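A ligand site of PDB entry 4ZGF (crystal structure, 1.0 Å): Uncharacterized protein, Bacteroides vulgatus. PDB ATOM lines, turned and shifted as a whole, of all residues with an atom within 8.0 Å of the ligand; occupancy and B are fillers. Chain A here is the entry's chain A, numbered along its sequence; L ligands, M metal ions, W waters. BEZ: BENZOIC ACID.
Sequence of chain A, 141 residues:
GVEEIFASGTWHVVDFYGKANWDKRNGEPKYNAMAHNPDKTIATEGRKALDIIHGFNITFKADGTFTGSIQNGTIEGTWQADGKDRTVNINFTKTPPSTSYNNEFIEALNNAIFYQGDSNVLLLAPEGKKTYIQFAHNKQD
Val 121 touches the ligand.
Ala 136 touches the ligand (CB to C1, 3.4 Å).
Hydrophobic or aromatic side chains within 4 Å of the ligand: Val 121 and Ala 136.
Within 4 Å of the ligand: Val 121, Ala 136, Asn 138 and Gln 140.
The nearest printed residue that does not touch the ligand is Val 14 (4.02 Å).
Water W2 lies within hydrogen-bond range of the backbone carbonyl oxygen of Asn 120 (2.7 Å), an oxygen (O2) of the ligand (2.8 Å) and the backbone NH of His 137 (2.8 Å).
The backbone carbonyl oxygen (O) of Asn 138 is in hydrogen-bond range of the side-chain amide nitrogen (NE2) of Gln 140.
The backbone carbonyl oxygen (O) of Ala 136 lies within hydrogen-bond range of the backbone NH (N) of His 12, 2.8 Å away.
N of Val 121 is in hydrogen-bond range of OD1 of Asp 118, at 3.0 Å.
The side-chain amide nitrogen (NE2) of Gln 140 lies within hydrogen-bond range of an oxygen (O1) of the ligand (2.8 Å).
The side-chain amide nitrogen (ND2) of Asn 138 is in hydrogen-bond range of an oxygen (O2) of the ligand.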
ATOM      1  N   TRP A  11      13.873   0.983   4.643  1.00  0.00           N
ATOM      2  CA  TRP A  11      13.237   2.100   5.308  1.00  0.00           C
ATOM      3  C   TRP A  11      11.731   2.051   5.057  1.00  0.00           C
ATOM      4  O   TRP A  11      11.284   1.987   3.906  1.00  0.00           O
ATOM      5  CB  TRP A  11      13.820   3.429   4.795  1.00  0.00           C
ATOM      6  CG  TRP A  11      15.204   3.759   5.258  1.00  0.00           C
ATOM      7  CD1 TRP A  11      16.316   3.790   4.482  1.00  0.00           C
ATOM      8  CD2 TRP A  11      15.633   4.126   6.585  1.00  0.00           C
ATOM      9  NE1 TRP A  11      17.410   4.195   5.213  1.00  0.00           N
ATOM     10  CE2 TRP A  11      17.008   4.429   6.507  1.00  0.00           C
ATOM     11  CE3 TRP A  11      14.988   4.236   7.822  1.00  0.00           C
ATOM     12  CZ2 TRP A  11      17.738   4.853   7.617  1.00  0.00           C
ATOM     13  CZ3 TRP A  11      15.726   4.653   8.909  1.00  0.00           C
ATOM     14  CH2 TRP A  11      17.070   4.958   8.802  1.00  0.00           C
ATOM     15  N   HIS A  12      10.949   2.104   6.138  1.00  0.00           N
ATOM     16  CA  HIS A  12       9.498   2.000   6.130  1.00  0.00           C
ATOM     17  C   HIS A  12       8.890   3.324   6.556  1.00  0.00           C
ATOM     18  O   HIS A  12       9.357   3.938   7.519  1.00  0.00           O
ATOM     19  CB  HIS A  12       9.060   0.899   7.117  1.00  0.00           C
ATOM     20  CG  HIS A  12       9.536  -0.459   6.788  1.00  0.00           C
ATOM     21  ND1 HIS A  12       8.787  -1.342   6.052  1.00  0.00           N
ATOM     22  CD2 HIS A  12      10.703  -1.090   7.107  1.00  0.00           C
ATOM     23  CE1 HIS A  12       9.469  -2.464   5.951  1.00  0.00           C
ATOM     24  NE2 HIS A  12      10.630  -2.335   6.574  1.00  0.00           N
ATOM     25  N   VAL A  13       7.820   3.762   5.892  1.00  0.00           N
ATOM     26  CA  VAL A  13       7.237   5.070   6.241  1.00  0.00           C
ATOM     27  C   VAL A  13       6.587   5.030   7.628  1.00  0.00           C
ATOM     28  O   VAL A  13       5.827   4.138   7.989  1.00  0.00           O
ATOM     29  CB  VAL A  13       6.196   5.481   5.190  1.00  0.00           C
ATOM     30  CG1 VAL A  13       5.401   6.697   5.623  1.00  0.00           C
ATOM     31  CG2 VAL A  13       6.874   5.770   3.873  1.00  0.00           C
ATOM     32  N   VAL A  14       6.917   6.087   8.390  1.00  0.00           N
ATOM     33  CA  VAL A  14       6.253   6.399   9.664  1.00  0.00           C
ATOM     34  C   VAL A  14       5.095   7.358   9.403  1.00  0.00           C
ATOM     35  O   VAL A  14       3.939   7.037   9.679  1.00  0.00           O
ATOM     36  CB  VAL A  14       7.257   6.922  10.702  1.00  0.00           C
ATOM     37  CG1 VAL A  14       6.545   7.321  11.988  1.00  0.00           C
ATOM     38  CG2 VAL A  14       8.347   5.909  10.972  1.00  0.00           C
ATOM     39  N   ASP A  15       5.388   8.563   8.905  1.00  0.00           N
ATOM     40  CA  ASP A  15       4.322   9.543   8.586  1.00  0.00           C
ATOM     41  C   ASP A  15       4.964  10.671   7.788  1.00  0.00           C
ATOM     42  O   ASP A  15       6.198  10.730   7.603  1.00  0.00           O
ATOM     43  CB  ASP A  15       3.672  10.081   9.904  1.00  0.00           C
ATOM     44  CG  ASP A  15       2.198  10.480   9.801  1.00  0.00           C
ATOM     45  OD1 ASP A  15       1.730  10.815   8.694  1.00  0.00           O
ATOM     46  OD2 ASP A  15       1.552  10.492  10.881  1.00  0.00           O
ATOM     47  N   TYR A  17       5.157  14.807   7.970  1.00  0.00           N
ATOM     48  CA  TYR A  17       5.155  15.763   9.072  1.00  0.00           C
ATOM     49  C   TYR A  17       5.041  17.175   8.536  1.00  0.00           C
ATOM     50  O   TYR A  17       5.705  17.535   7.545  1.00  0.00           O
ATOM     51  CB  TYR A  17       6.438  15.625   9.908  1.00  0.00           C
ATOM     52  CG  TYR A  17       6.470  14.329  10.709  1.00  0.00           C
ATOM     53  CD1 TYR A  17       6.648  13.105  10.096  1.00  0.00           C
ATOM     54  CD2 TYR A  17       6.303  14.342  12.081  1.00  0.00           C
ATOM     55  CE1 TYR A  17       6.642  11.928  10.813  1.00  0.00           C
ATOM     56  CE2 TYR A  17       6.320  13.175  12.831  1.00  0.00           C
ATOM     57  CZ  TYR A  17       6.470  11.972  12.193  1.00  0.00           C
ATOM     58  OH  TYR A  17       6.468  10.764  12.861  1.00  0.00           O
ATOM     59  N   ARG A  25      14.343  18.476  14.616  1.00  0.00           N
ATOM     60  CA  ARG A  25      13.751  17.191  14.152  1.00  0.00           C
ATOM     61  C   ARG A  25      12.368  16.959  14.730  1.00  0.00           C
ATOM     62  O   ARG A  25      12.017  15.862  15.162  1.00  0.00           O
ATOM     63  CB  ARG A  25      14.696  15.994  14.287  1.00  0.00           C
ATOM     64  CG  ARG A  25      15.446  15.880  15.547  1.00  0.00           C
ATOM     65  CD  ARG A  25      16.428  14.725  15.476  1.00  0.00           C
ATOM     66  NE  ARG A  25      15.817  13.444  15.671  1.00  0.00           N
ATOM     67  CZ  ARG A  25      16.442  12.253  15.637  1.00  0.00           C
ATOM     68  NH1 ARG A  25      17.664  12.114  15.157  1.00  0.00           N
ATOM     69  NH2 ARG A  25      15.806  11.198  16.123  1.00  0.00           N
ATOM     70  N   ASP A 118      19.481   8.815  12.088  1.00  0.00           N
ATOM     71  CA  ASP A 118      20.258   8.068  13.062  1.00  0.00           C
ATOM     72  C   ASP A 118      20.011   6.581  12.834  1.00  0.00           C
ATOM     73  O   ASP A 118      19.462   6.196  11.793  1.00  0.00           O
ATOM     74  CB  ASP A 118      20.018   8.529  14.522  1.00  0.00           C
ATOM     75  CG  ASP A 118      18.578   8.426  14.987  1.00  0.00           C
ATOM     76  OD1 ASP A 118      17.877   7.496  14.548  1.00  0.00           O
ATOM     77  OD2 ASP A 118      18.223   9.248  15.876  1.00  0.00           O
ATOM     78  N   SER A 119      20.442   5.709  13.731  1.00  0.00           N
ATOM     79  CA  SER A 119      20.262   4.270  13.473  1.00  0.00           C
ATOM     80  C   SER A 119      18.758   3.872  13.468  1.00  0.00           C
ATOM     81  O   SER A 119      18.462   2.727  13.054  1.00  0.00           O
ATOM     82  CB  SER A 119      20.986   3.479  14.540  1.00  0.00           C
ATOM     83  OG  SER A 119      20.429   3.850  15.756  1.00  0.00           O
ATOM     84  N   ASN A 120      17.840   4.708  13.966  1.00  0.00           N
ATOM     85  CA  ASN A 120      16.397   4.373  14.006  1.00  0.00           C
ATOM     86  C   ASN A 120      15.577   5.055  12.934  1.00  0.00           C
ATOM     87  O   ASN A 120      14.577   4.495  12.535  1.00  0.00           O
ATOM     88  CB  ASN A 120      15.663   4.746  15.327  1.00  0.00           C
ATOM     89  CG  ASN A 120      16.189   4.076  16.539  1.00  0.00           C
ATOM     90  OD1 ASN A 120      16.256   2.840  16.624  1.00  0.00           O
ATOM     91  ND2 ASN A 120      16.515   4.890  17.541  1.00  0.00           N
ATOM     92  N   VAL A 121      15.949   6.285  12.544  1.00  0.00           N
ATOM     93  CA  VAL A 121      15.080   7.113  11.724  1.00  0.00           C
ATOM     94  C   VAL A 121      15.869   7.815  10.607  1.00  0.00           C
ATOM     95  O   VAL A 121      17.050   8.115  10.716  1.00  0.00           O
ATOM     96  CB  VAL A 121      14.248   8.164  12.529  1.00  0.00           C
ATOM     97  CG1 VAL A 121      13.303   7.465  13.515  1.00  0.00           C
ATOM     98  CG2 VAL A 121      15.129   9.212  13.190  1.00  0.00           C
ATOM     99  N   LEU A 122      15.134   8.104   9.564  1.00  0.00           N
ATOM    100  CA  LEU A 122      15.583   8.919   8.417  1.00  0.00           C
ATOM    101  C   LEU A 122      14.505   9.940   8.148  1.00  0.00           C
ATOM    102  O   LEU A 122      13.332   9.580   7.984  1.00  0.00           O
ATOM    103  CB  LEU A 122      15.813   8.043   7.177  1.00  0.00           C
ATOM    104  CG  LEU A 122      16.217   8.789   5.911  1.00  0.00           C
ATOM    105  CD1 LEU A 122      17.549   9.496   6.043  1.00  0.00           C
ATOM    106  CD2 LEU A 122      16.232   7.803   4.750  1.00  0.00           C
ATOM    107  N   GLN A 134       9.264  10.873   7.395  1.00  0.00           N
ATOM    108  CA  GLN A 134      10.087  10.109   8.324  1.00  0.00           C
ATOM    109  C   GLN A 134       9.919   8.617   8.062  1.00  0.00           C
ATOM    110  O   GLN A 134       8.790   8.138   7.890  1.00  0.00           O
ATOM    111  CB  GLN A 134       9.759  10.451   9.776  1.00  0.00           C
ATOM    112  CG  GLN A 134      10.700   9.784  10.788  1.00  0.00           C
ATOM    113  CD  GLN A 134      10.528  10.228  12.233  1.00  0.00           C
ATOM    114  OE1 GLN A 134       9.422  10.239  12.783  1.00  0.00           O
ATOM    115  NE2 GLN A 134      11.635  10.537  12.879  1.00  0.00           N
ATOM    116  N   PHE A 135      11.054   7.922   8.099  1.00  0.00           N
ATOM    117  CA  PHE A 135      11.099   6.461   7.966  1.00  0.00           C
ATOM    118  C   PHE A 135      11.764   5.837   9.198  1.00  0.00           C
ATOM    119  O   PHE A 135      12.538   6.486   9.898  1.00  0.00           O
ATOM    120  CB  PHE A 135      11.988   6.064   6.771  1.00  0.00           C
ATOM    121  CG  PHE A 135      11.557   6.593   5.432  1.00  0.00           C
ATOM    122  CD1 PHE A 135      11.950   7.841   4.995  1.00  0.00           C
ATOM    123  CD2 PHE A 135      10.797   5.817   4.557  1.00  0.00           C
ATOM    124  CE1 PHE A 135      11.581   8.282   3.727  1.00  0.00           C
ATOM    125  CE2 PHE A 135      10.451   6.270   3.312  1.00  0.00           C
ATOM    126  CZ  PHE A 135      10.861   7.488   2.899  1.00  0.00           C
ATOM    127  N   ALA A 136      11.476   4.560   9.380  1.00  0.00           N
ATOM    128  CA  ALA A 136      12.118   3.711  10.393  1.00  0.00           C
ATOM    129  C   ALA A 136      12.555   2.394   9.745  1.00  0.00           C
ATOM    130  O   ALA A 136      12.163   2.077   8.615  1.00  0.00           O
ATOM    131  CB  ALA A 136      11.137   3.417  11.538  1.00  0.00           C
ATOM    132  N   HIS A 137      13.342   1.590  10.469  1.00  0.00           N
ATOM    133  CA  HIS A 137      13.788   0.309   9.922  1.00  0.00           C
ATOM    134  C   HIS A 137      12.872  -0.873  10.207  1.00  0.00           C
ATOM    135  O   HIS A 137      13.179  -1.996   9.874  1.00  0.00           O
ATOM    136  CB  HIS A 137      15.187  -0.025  10.371  1.00  0.00           C
ATOM    137  CG  HIS A 137      16.267   0.740   9.677  1.00  0.00           C
ATOM    138  ND1 HIS A 137      16.362   0.793   8.290  1.00  0.00           N
ATOM    139  CD2 HIS A 137      17.319   1.431  10.148  1.00  0.00           C
ATOM    140  CE1 HIS A 137      17.445   1.460   7.963  1.00  0.00           C
ATOM    141  NE2 HIS A 137      18.032   1.880   9.054  1.00  0.00           N
ATOM    142  N   ASN A 138      11.702  -0.607  10.777  1.00  0.00           N
ATOM    143  CA  ASN A 138      10.660  -1.590  11.008  1.00  0.00           C
ATOM    144  C   ASN A 138       9.360  -1.096  10.432  1.00  0.00           C
ATOM    145  O   ASN A 138       9.072   0.108  10.496  1.00  0.00           O
ATOM    146  CB  ASN A 138      10.479  -1.850  12.490  1.00  0.00           C
ATOM    147  CG  ASN A 138      11.725  -2.438  13.055  1.00  0.00           C
ATOM    148  OD1 ASN A 138      12.070  -3.602  12.784  1.00  0.00           O
ATOM    149  ND2 ASN A 138      12.483  -1.620  13.755  1.00  0.00           N
ATOM    150  N   LYS A 139       8.574  -2.022   9.902  1.00  0.00           N
ATOM    151  CA  LYS A 139       7.228  -1.676   9.455  1.00  0.00           C
ATOM    152  C   LYS A 139       6.382  -1.259  10.624  1.00  0.00           C
ATOM    153  O   LYS A 139       6.356  -1.908  11.672  1.00  0.00           O
ATOM    154  CB  LYS A 139       6.636  -2.876   8.724  1.00  0.00           C
ATOM    155  CG  LYS A 139       5.312  -2.582   8.049  1.00  0.00           C
ATOM    156  CD  LYS A 139       4.830  -3.756   7.220  1.00  0.00           C
ATOM    157  CE  LYS A 139       3.554  -3.454   6.474  1.00  0.00           C
ATOM    158  NZ  LYS A 139       3.271  -4.460   5.467  1.00  0.00           N
ATOM    159  N   GLN A 140       5.674  -0.157  10.473  1.00  0.00           N
ATOM    160  CA  GLN A 140       4.757   0.305  11.499  1.00  0.00           C
ATOM    161  C   GLN A 140       3.490  -0.540  11.467  1.00  0.00           C
ATOM    162  O   GLN A 140       3.086  -1.039  10.417  1.00  0.00           O
ATOM    163  CB  GLN A 140       4.425   1.778  11.289  1.00  0.00           C
ATOM    164  CG  GLN A 140       5.642   2.682  11.150  1.00  0.00           C
ATOM    165  CD  GLN A 140       6.562   2.579  12.338  1.00  0.00           C
ATOM    166  OE1 GLN A 140       6.260   3.152  13.414  1.00  0.00           O
ATOM    167  NE2 GLN A 140       7.631   1.823  12.238  1.00  0.00           N
ATOM    168  N   ASP A 141       2.866  -0.689  12.642  1.00  0.00           N
ATOM    169  CA  ASP A 141       1.738  -1.612  12.805  1.00  0.00           C
ATOM    170  C   ASP A 141       0.766  -1.200  13.902  1.00  0.00           C
ATOM    171  O   ASP A 141       1.045  -0.207  14.618  1.00  0.00           O
ATOM    172  CB  ASP A 141       2.264  -3.022  13.059  1.00  0.00           C
ATOM    173  CG  ASP A 141       3.143  -3.135  14.276  1.00  0.00           C
ATOM    174  OD1 ASP A 141       3.090  -2.256  15.165  1.00  0.00           O
ATOM    175  OD2 ASP A 141       3.948  -4.107  14.384  1.00  0.00           O
ATOM    176  OXT ASP A 141      -0.251  -1.914  14.032  1.00  0.00           O
HETATM  177  C   BEZ L   1      10.586   1.646  14.556  1.00  0.00           C
HETATM  178  O1  BEZ L   1       9.469   1.075  14.279  1.00  0.00           O
HETATM  179  O2  BEZ L   1      11.724   1.046  14.584  1.00  0.00           O
HETATM  180  C1  BEZ L   1      10.562   3.118  14.897  1.00  0.00           C
HETATM  181  C2  BEZ L   1      11.712   3.757  15.436  1.00  0.00           C
HETATM  182  C3  BEZ L   1      11.659   5.130  15.682  1.00  0.00           C
HETATM  183  C4  BEZ L   1      10.522   5.898  15.385  1.00  0.00           C
HETATM  184  C5  BEZ L   1       9.343   5.270  14.818  1.00  0.00           C
HETATM  185  C6  BEZ L   1       9.417   3.893  14.612  1.00  0.00           C
HETATM  186 CA    CA M   1       4.955  -3.348  16.486  1.00  0.00          CA
HETATM  187 CA    CA M   2       2.564  -0.340  16.594  1.00  0.00          CA
HETATM  188  O   HOH W   1       8.662  -1.409  15.115  1.00  0.00           O
HETATM  189  O   HOH W   2      14.005   1.941  13.208  1.00  0.00           O
